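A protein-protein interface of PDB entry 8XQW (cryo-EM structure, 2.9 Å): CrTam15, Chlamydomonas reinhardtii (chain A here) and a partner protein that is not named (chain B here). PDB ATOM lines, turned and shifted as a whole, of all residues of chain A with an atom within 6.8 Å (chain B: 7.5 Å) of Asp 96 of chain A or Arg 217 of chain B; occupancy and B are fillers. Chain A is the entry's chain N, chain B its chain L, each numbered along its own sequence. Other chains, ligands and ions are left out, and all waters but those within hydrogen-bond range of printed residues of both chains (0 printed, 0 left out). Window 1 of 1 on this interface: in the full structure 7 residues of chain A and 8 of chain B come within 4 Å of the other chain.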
ATOM      1  N   PRO A  94      31.831   8.706 -18.360  1.00  0.00           N
ATOM      2  CA  PRO A  94      31.993   7.280 -18.576  1.00  0.00           C
ATOM      3  C   PRO A  94      31.705   6.926 -20.021  1.00  0.00           C
ATOM      4  O   PRO A  94      31.203   7.763 -20.781  1.00  0.00           O
ATOM      5  CB  PRO A  94      30.943   6.680 -17.641  1.00  0.00           C
ATOM      6  CG  PRO A  94      29.872   7.699 -17.637  1.00  0.00           C
ATOM      7  CD  PRO A  94      30.530   9.032 -17.762  1.00  0.00           C
ATOM      8  N   PRO A  95      32.010   5.707 -20.446  1.00  0.00           N
ATOM      9  CA  PRO A  95      31.609   5.289 -21.787  1.00  0.00           C
ATOM     10  C   PRO A  95      30.102   5.130 -21.878  1.00  0.00           C
ATOM     11  O   PRO A  95      29.422   4.805 -20.907  1.00  0.00           O
ATOM     12  CB  PRO A  95      32.322   3.947 -21.972  1.00  0.00           C
ATOM     13  CG  PRO A  95      33.405   3.956 -20.977  1.00  0.00           C
ATOM     14  CD  PRO A  95      32.875   4.709 -19.810  1.00  0.00           C
ATOM     15  N   ASP A  96      29.580   5.363 -23.072  1.00  0.00           N
ATOM     16  CA  ASP A  96      28.156   5.256 -23.322  1.00  0.00           C
ATOM     17  C   ASP A  96      27.946   4.321 -24.496  1.00  0.00           C
ATOM     18  O   ASP A  96      28.718   4.344 -25.451  1.00  0.00           O
ATOM     19  CB  ASP A  96      27.546   6.622 -23.613  1.00  0.00           C
ATOM     20  CG  ASP A  96      26.048   6.605 -23.582  1.00  0.00           C
ATOM     21  OD1 ASP A  96      25.470   5.516 -23.424  1.00  0.00           O
ATOM     22  OD2 ASP A  96      25.442   7.683 -23.717  1.00  0.00           O
ATOM     23  N   ARG A  97      26.907   3.504 -24.429  1.00  0.00           N
ATOM     24  CA  ARG A  97      26.705   2.508 -25.464  1.00  0.00           C
ATOM     25  C   ARG A  97      25.716   2.942 -26.524  1.00  0.00           C
ATOM     26  O   ARG A  97      25.655   2.316 -27.580  1.00  0.00           O
ATOM     27  CB  ARG A  97      26.244   1.190 -24.848  1.00  0.00           C
ATOM     28  CG  ARG A  97      24.807   1.135 -24.455  1.00  0.00           C
ATOM     29  CD  ARG A  97      24.405  -0.280 -24.202  1.00  0.00           C
ATOM     30  NE  ARG A  97      22.966  -0.432 -24.073  1.00  0.00           N
ATOM     31  CZ  ARG A  97      22.342  -0.591 -22.916  1.00  0.00           C
ATOM     32  NH1 ARG A  97      21.034  -0.735 -22.876  1.00  0.00           N
ATOM     33  NH2 ARG A  97      23.033  -0.609 -21.797  1.00  0.00           N
ATOM     34  N   TYR A  98      24.937   3.981 -26.275  1.00  0.00           N
ATOM     35  CA  TYR A  98      24.109   4.539 -27.327  1.00  0.00           C
ATOM     36  C   TYR A  98      24.870   5.502 -28.213  1.00  0.00           C
ATOM     37  O   TYR A  98      24.357   5.881 -29.265  1.00  0.00           O
ATOM     38  CB  TYR A  98      22.911   5.256 -26.736  1.00  0.00           C
ATOM     39  CG  TYR A  98      21.942   4.345 -26.063  1.00  0.00           C
ATOM     40  CD1 TYR A  98      22.077   4.037 -24.738  1.00  0.00           C
ATOM     41  CD2 TYR A  98      20.884   3.806 -26.748  1.00  0.00           C
ATOM     42  CE1 TYR A  98      21.199   3.217 -24.117  1.00  0.00           C
ATOM     43  CE2 TYR A  98      20.003   2.980 -26.127  1.00  0.00           C
ATOM     44  CZ  TYR A  98      20.168   2.696 -24.810  1.00  0.00           C
ATOM     45  OH  TYR A  98      19.302   1.869 -24.163  1.00  0.00           O
ATOM     46  N   TRP A  99      26.074   5.896 -27.821  1.00  0.00           N
ATOM     47  CA  TRP A  99      26.852   6.901 -28.539  1.00  0.00           C
ATOM     48  C   TRP A  99      28.313   6.504 -28.553  1.00  0.00           C
ATOM     49  O   TRP A  99      29.140   7.108 -27.865  1.00  0.00           O
ATOM     50  CB  TRP A  99      26.694   8.274 -27.894  1.00  0.00           C
ATOM     51  CG  TRP A  99      25.318   8.756 -27.921  1.00  0.00           C
ATOM     52  CD1 TRP A  99      24.438   8.775 -26.891  1.00  0.00           C
ATOM     53  CD2 TRP A  99      24.636   9.295 -29.044  1.00  0.00           C
ATOM     54  NE1 TRP A  99      23.240   9.295 -27.302  1.00  0.00           N
ATOM     55  CE2 TRP A  99      23.340   9.620 -28.627  1.00  0.00           C
ATOM     56  CE3 TRP A  99      24.997   9.534 -30.368  1.00  0.00           C
ATOM     57  CZ2 TRP A  99      22.404  10.168 -29.483  1.00  0.00           C
ATOM     58  CZ3 TRP A  99      24.070  10.075 -31.213  1.00  0.00           C
ATOM     59  CH2 TRP A  99      22.791  10.390 -30.771  1.00  0.00           C
ATOM     60  N   PRO A 100      28.677   5.496 -29.336  1.00  0.00           N
ATOM     61  CA  PRO A 100      30.093   5.183 -29.504  1.00  0.00           C
ATOM     62  C   PRO A 100      30.821   6.348 -30.151  1.00  0.00           C
ATOM     63  O   PRO A 100      30.223   7.330 -30.587  1.00  0.00           O
ATOM     64  CB  PRO A 100      30.078   3.956 -30.413  1.00  0.00           C
ATOM     65  CG  PRO A 100      28.719   3.441 -30.342  1.00  0.00           C
ATOM     66  CD  PRO A 100      27.834   4.599 -30.130  1.00  0.00           C
ATOM     67  N   THR A 101      32.141   6.231 -30.222  1.00  0.00           N
ATOM     68  CA  THR A 101      32.938   7.332 -30.739  1.00  0.00           C
ATOM     69  C   THR A 101      33.105   7.304 -32.248  1.00  0.00           C
ATOM     70  O   THR A 101      33.511   8.314 -32.819  1.00  0.00           O
ATOM     71  CB  THR A 101      34.313   7.336 -30.087  1.00  0.00           C
ATOM     72  OG1 THR A 101      34.787   5.991 -29.974  1.00  0.00           O
ATOM     73  CG2 THR A 101      34.230   7.943 -28.710  1.00  0.00           C
ATOM     74  N   TRP B 209      23.925   4.708 -10.249  1.00  0.00           N
ATOM     75  CA  TRP B 209      22.773   5.314 -10.909  1.00  0.00           C
ATOM     76  C   TRP B 209      22.475   4.663 -12.243  1.00  0.00           C
ATOM     77  O   TRP B 209      21.316   4.566 -12.631  1.00  0.00           O
ATOM     78  CB  TRP B 209      23.005   6.811 -11.100  1.00  0.00           C
ATOM     79  CG  TRP B 209      22.105   7.486 -12.093  1.00  0.00           C
ATOM     80  CD1 TRP B 209      20.779   7.728 -11.964  1.00  0.00           C
ATOM     81  CD2 TRP B 209      22.485   8.036 -13.353  1.00  0.00           C
ATOM     82  NE1 TRP B 209      20.305   8.375 -13.069  1.00  0.00           N
ATOM     83  CE2 TRP B 209      21.340   8.579 -13.934  1.00  0.00           C
ATOM     84  CE3 TRP B 209      23.688   8.120 -14.044  1.00  0.00           C
ATOM     85  CZ2 TRP B 209      21.357   9.179 -15.170  1.00  0.00           C
ATOM     86  CZ3 TRP B 209      23.700   8.717 -15.265  1.00  0.00           C
ATOM     87  CH2 TRP B 209      22.549   9.244 -15.815  1.00  0.00           C
ATOM     88  N   ARG B 210      23.491   4.200 -12.957  1.00  0.00           N
ATOM     89  CA  ARG B 210      23.229   3.596 -14.249  1.00  0.00           C
ATOM     90  C   ARG B 210      22.621   2.223 -14.113  1.00  0.00           C
ATOM     91  O   ARG B 210      21.933   1.766 -15.024  1.00  0.00           O
ATOM     92  CB  ARG B 210      24.505   3.499 -15.057  1.00  0.00           C
ATOM     93  CG  ARG B 210      24.694   4.639 -15.974  1.00  0.00           C
ATOM     94  CD  ARG B 210      25.446   4.196 -17.174  1.00  0.00           C
ATOM     95  NE  ARG B 210      25.823   5.330 -17.989  1.00  0.00           N
ATOM     96  CZ  ARG B 210      26.809   5.299 -18.869  1.00  0.00           C
ATOM     97  NH1 ARG B 210      27.508   4.187 -19.041  1.00  0.00           N
ATOM     98  NH2 ARG B 210      27.090   6.380 -19.570  1.00  0.00           N
ATOM     99  N   ASN B 211      22.879   1.534 -13.007  1.00  0.00           N
ATOM    100  CA  ASN B 211      22.245   0.230 -12.862  1.00  0.00           C
ATOM    101  C   ASN B 211      20.796   0.306 -12.419  1.00  0.00           C
ATOM    102  O   ASN B 211      20.113  -0.717 -12.448  1.00  0.00           O
ATOM    103  CB  ASN B 211      23.025  -0.624 -11.882  1.00  0.00           C
ATOM    104  CG  ASN B 211      24.160  -1.328 -12.538  1.00  0.00           C
ATOM    105  OD1 ASN B 211      24.081  -1.700 -13.697  1.00  0.00           O
ATOM    106  ND2 ASN B 211      25.237  -1.502 -11.811  1.00  0.00           N
ATOM    107  N   SER B 213      18.564   2.742 -13.705  1.00  0.00           N
ATOM    108  CA  SER B 213      17.844   3.638 -14.592  1.00  0.00           C
ATOM    109  C   SER B 213      17.914   3.169 -16.025  1.00  0.00           C
ATOM    110  O   SER B 213      18.235   3.943 -16.923  1.00  0.00           O
ATOM    111  CB  SER B 213      18.386   5.052 -14.488  1.00  0.00           C
ATOM    112  OG  SER B 213      17.889   5.675 -13.325  1.00  0.00           O
ATOM    113  N   GLU B 214      17.618   1.903 -16.275  1.00  0.00           N
ATOM    114  CA  GLU B 214      17.715   1.387 -17.629  1.00  0.00           C
ATOM    115  C   GLU B 214      16.463   1.655 -18.445  1.00  0.00           C
ATOM    116  O   GLU B 214      16.558   1.966 -19.640  1.00  0.00           O
ATOM    117  CB  GLU B 214      18.006  -0.101 -17.581  1.00  0.00           C
ATOM    118  CG  GLU B 214      19.357  -0.426 -17.008  1.00  0.00           C
ATOM    119  CD  GLU B 214      20.477  -0.316 -18.031  1.00  0.00           C
ATOM    120  OE1 GLU B 214      20.741  -1.312 -18.737  1.00  0.00           O
ATOM    121  OE2 GLU B 214      21.100   0.760 -18.128  1.00  0.00           O
ATOM    122  N   ASN B 215      15.287   1.549 -17.828  1.00  0.00           N
ATOM    123  CA  ASN B 215      14.049   1.817 -18.543  1.00  0.00           C
ATOM    124  C   ASN B 215      13.964   3.275 -18.953  1.00  0.00           C
ATOM    125  O   ASN B 215      13.575   3.594 -20.076  1.00  0.00           O
ATOM    126  CB  ASN B 215      12.856   1.449 -17.681  1.00  0.00           C
ATOM    127  CG  ASN B 215      12.852   0.018 -17.280  1.00  0.00           C
ATOM    128  OD1 ASN B 215      12.385  -0.837 -18.008  1.00  0.00           O
ATOM    129  ND2 ASN B 215      13.368  -0.259 -16.106  1.00  0.00           N
ATOM    130  N   GLU B 216      14.314   4.179 -18.050  1.00  0.00           N
ATOM    131  CA  GLU B 216      14.235   5.592 -18.376  1.00  0.00           C
ATOM    132  C   GLU B 216      15.286   5.986 -19.390  1.00  0.00           C
ATOM    133  O   GLU B 216      15.049   6.865 -20.219  1.00  0.00           O
ATOM    134  CB  GLU B 216      14.375   6.416 -17.110  1.00  0.00           C
ATOM    135  CG  GLU B 216      13.316   6.128 -16.101  1.00  0.00           C
ATOM    136  CD  GLU B 216      13.668   4.987 -15.198  1.00  0.00           C
ATOM    137  OE1 GLU B 216      14.665   4.321 -15.477  1.00  0.00           O
ATOM    138  OE2 GLU B 216      12.963   4.751 -14.206  1.00  0.00           O
ATOM    139  N   ARG B 217      16.442   5.351 -19.350  1.00  0.00           N
ATOM    140  CA  ARG B 217      17.467   5.631 -20.338  1.00  0.00           C
ATOM    141  C   ARG B 217      16.996   5.231 -21.723  1.00  0.00           C
ATOM    142  O   ARG B 217      17.127   5.999 -22.676  1.00  0.00           O
ATOM    143  CB  ARG B 217      18.739   4.895 -19.961  1.00  0.00           C
ATOM    144  CG  ARG B 217      19.986   5.383 -20.605  1.00  0.00           C
ATOM    145  CD  ARG B 217      21.105   4.475 -20.217  1.00  0.00           C
ATOM    146  NE  ARG B 217      22.273   4.643 -21.063  1.00  0.00           N
ATOM    147  CZ  ARG B 217      23.316   3.828 -21.049  1.00  0.00           C
ATOM    148  NH1 ARG B 217      23.329   2.796 -20.231  1.00  0.00           N
ATOM    149  NH2 ARG B 217      24.343   4.046 -21.843  1.00  0.00           N
ATOM    150  N   TRP B 218      16.427   4.035 -21.858  1.00  0.00           N
ATOM    151  CA  TRP B 218      15.919   3.655 -23.168  1.00  0.00           C
ATOM    152  C   TRP B 218      14.771   4.542 -23.597  1.00  0.00           C
ATOM    153  O   TRP B 218      14.665   4.876 -24.773  1.00  0.00           O
ATOM    154  CB  TRP B 218      15.483   2.201 -23.174  1.00  0.00           C
ATOM    155  CG  TRP B 218      15.106   1.687 -24.514  1.00  0.00           C
ATOM    156  CD1 TRP B 218      15.933   1.183 -25.445  1.00  0.00           C
ATOM    157  CD2 TRP B 218      13.794   1.608 -25.062  1.00  0.00           C
ATOM    158  NE1 TRP B 218      15.231   0.798 -26.543  1.00  0.00           N
ATOM    159  CE2 TRP B 218      13.908   1.048 -26.326  1.00  0.00           C
ATOM    160  CE3 TRP B 218      12.532   1.962 -24.599  1.00  0.00           C
ATOM    161  CZ2 TRP B 218      12.818   0.839 -27.137  1.00  0.00           C
ATOM    162  CZ3 TRP B 218      11.462   1.747 -25.396  1.00  0.00           C
ATOM    163  CH2 TRP B 218      11.604   1.193 -26.649  1.00  0.00           C
ATOM    164  N   PHE B 219      13.910   4.951 -22.671  1.00  0.00           N
ATOM    165  CA  PHE B 219      12.802   5.813 -23.051  1.00  0.00           C
ATOM    166  C   PHE B 219      13.304   7.132 -23.604  1.00  0.00           C
ATOM    167  O   PHE B 219      12.885   7.567 -24.676  1.00  0.00           O
ATOM    168  CB  PHE B 219      11.890   6.052 -21.865  1.00  0.00           C
ATOM    169  CG  PHE B 219      10.817   7.042 -22.133  1.00  0.00           C
ATOM    170  CD1 PHE B 219       9.731   6.705 -22.891  1.00  0.00           C
ATOM    171  CD2 PHE B 219      10.884   8.306 -21.621  1.00  0.00           C
ATOM    172  CE1 PHE B 219       8.757   7.614 -23.135  1.00  0.00           C
ATOM    173  CE2 PHE B 219       9.910   9.210 -21.871  1.00  0.00           C
ATOM    174  CZ  PHE B 219       8.845   8.864 -22.619  1.00  0.00           C
ATOM    175  N   TRP B 220      14.212   7.784 -22.897  1.00  0.00           N
ATOM    176  CA  TRP B 220      14.679   9.076 -23.364  1.00  0.00           C
ATOM    177  C   TRP B 220      15.617   8.977 -24.550  1.00  0.00           C
ATOM    178  O   TRP B 220      15.809   9.976 -25.238  1.00  0.00           O
ATOM    179  CB  TRP B 220      15.357   9.830 -22.229  1.00  0.00           C
ATOM    180  CG  TRP B 220      14.390  10.425 -21.292  1.00  0.00           C
ATOM    181  CD1 TRP B 220      14.212  10.093 -20.000  1.00  0.00           C
ATOM    182  CD2 TRP B 220      13.448  11.454 -21.575  1.00  0.00           C
ATOM    183  NE1 TRP B 220      13.217  10.844 -19.452  1.00  0.00           N
ATOM    184  CE2 TRP B 220      12.731  11.690 -20.403  1.00  0.00           C
ATOM    185  CE3 TRP B 220      13.137  12.196 -22.711  1.00  0.00           C
ATOM    186  CZ2 TRP B 220      11.731  12.637 -20.331  1.00  0.00           C
ATOM    187  CZ3 TRP B 220      12.154  13.128 -22.635  1.00  0.00           C
ATOM    188  CH2 TRP B 220      11.457  13.341 -21.459  1.00  0.00           C
ATOM    189  N   GLU B 221      16.193   7.816 -24.830  1.00  0.00           N
ATOM    190  CA  GLU B 221      17.109   7.741 -25.958  1.00  0.00           C
ATOM    191  C   GLU B 221      16.476   7.216 -27.232  1.00  0.00           C
ATOM    192  O   GLU B 221      16.897   7.611 -28.318  1.00  0.00           O
ATOM    193  CB  GLU B 221      18.303   6.857 -25.620  1.00  0.00           C
ATOM    194  CG  GLU B 221      19.182   7.396 -24.533  1.00  0.00           C
ATOM    195  CD  GLU B 221      20.175   8.400 -25.044  1.00  0.00           C
ATOM    196  OE1 GLU B 221      20.547   8.309 -26.228  1.00  0.00           O
ATOM    197  OE2 GLU B 221      20.584   9.281 -24.264  1.00  0.00           O
ATOM    198  N   VAL B 222      15.486   6.336 -27.147  1.00  0.00           N
ATOM    199  CA  VAL B 222      15.025   5.628 -28.333  1.00  0.00           C
ATOM    200  C   VAL B 222      13.539   5.840 -28.580  1.00  0.00           C
ATOM    201  O   VAL B 222      13.057   5.676 -29.701  1.00  0.00           O
ATOM    202  CB  VAL B 222      15.357   4.136 -28.209  1.00  0.00           C
ATOM    203  CG1 VAL B 222      14.869   3.385 -29.393  1.00  0.00           C
ATOM    204  CG2 VAL B 222      16.835   3.953 -28.096  1.00  0.00           C
ATOM    205  N   PHE B 223      12.799   6.238 -27.563  1.00  0.00           N
ATOM    206  CA  PHE B 223      11.352   6.241 -27.674  1.00  0.00           C
ATOM    207  C   PHE B 223      10.716   7.613 -27.594  1.00  0.00           C
ATOM    208  O   PHE B 223       9.660   7.812 -28.171  1.00  0.00           O
ATOM    209  CB  PHE B 223      10.759   5.361 -26.583  1.00  0.00           C
ATOM    210  CG  PHE B 223       9.327   5.040 -26.783  1.00  0.00           C
ATOM    211  CD1 PHE B 223       8.956   3.989 -27.568  1.00  0.00           C
ATOM    212  CD2 PHE B 223       8.353   5.773 -26.166  1.00  0.00           C
ATOM    213  CE1 PHE B 223       7.646   3.697 -27.748  1.00  0.00           C
ATOM    214  CE2 PHE B 223       7.047   5.477 -26.348  1.00  0.00           C
ATOM    215  CZ  PHE B 223       6.693   4.439 -27.133  1.00  0.00           C
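Pro 94 of chain A touches Arg 210 of chain B.
Arg 97 of chain A touches Arg 217 of chain B.
Arg 217 of chain B touches Tyr 98 of chain A.
Tyr 98 of chain A touches Trp 218 of chain B.
CB of Tyr 98 of chain A touches OE1 of Glu 221 of chain B, 3.9 Å away.
Tyr 98 of chain A touches Val 222 of chain B.
The side-chain carboxylate (OE2) of Glu 214 of chain B lies within salt-bridge range of the guanidinium group (NH1) of Arg 217 of chain B.
The side-chain carboxylate of Asp 96 of chain A is in hydrogen-bond range of the backbone NH of Tyr 98 of chain A, at 3.3 Å.
The guanidinium group (NH1) of Arg 97 of chain A is in hydrogen-bond range of the side-chain hydroxyl (OH) of Tyr 98 of chain A (3.4 Å).
Asp 96 of chain A touches just one residue of chain B: Arg 217.
Arg 217 of chain B touches three residues of chain A.
Printed residues of chain A within 4 Å of Val 222 of chain B: Tyr 98 (3.9 Å).
Of the printed residues of chain B, Pro 94 of chain A touches Arg 210 (3.6 Å).
Thr 101 of chain A touches none of the printed residues of chain B.
Pro 100 of chain A touches none of the printed residues of chain B.
The guanidinium group (NH1) of Arg 210 of chain B is in hydrogen-bond range of the backbone carbonyl oxygen (O) of Pro 95 of chain A, at 2.7 Å.
The side-chain carboxylate (OE1) of Glu 214 of chain B lies within salt-bridge range of the guanidinium group (NH2) of Arg 97 of chain A, at 3.9 Å.
OD1 of Asp 96 of chain A lies within salt-bridge range of NH2 of Arg 217 of chain B, 2.4 Å away.
NE1 of Trp 99 of chain A lies within hydrogen-bond range of OE1 of Glu 221 of chain B.
Hydrophobic or aromatic side chains of chain B within 4 Å of the printed part of chain A: Trp 218 and Val 222.
Of the 8 printed residues of chain A, 6 touch a printed residue of chain B.
Printed residues of chain A that touch a printed residue of chain B: Pro 94, Pro 95, Asp 96, Arg 97, Tyr 98 and Trp 99.
Among the printed residues, 10 pairs touch across the chains.
Among the printed residues, Asp or Glu carboxylates within 4 Å of a Lys or Arg side-chain nitrogen of the other chain: Asp 96 of chain A with Arg 217 of chain B and Arg 97 of chain A with Glu 214 of chain B.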
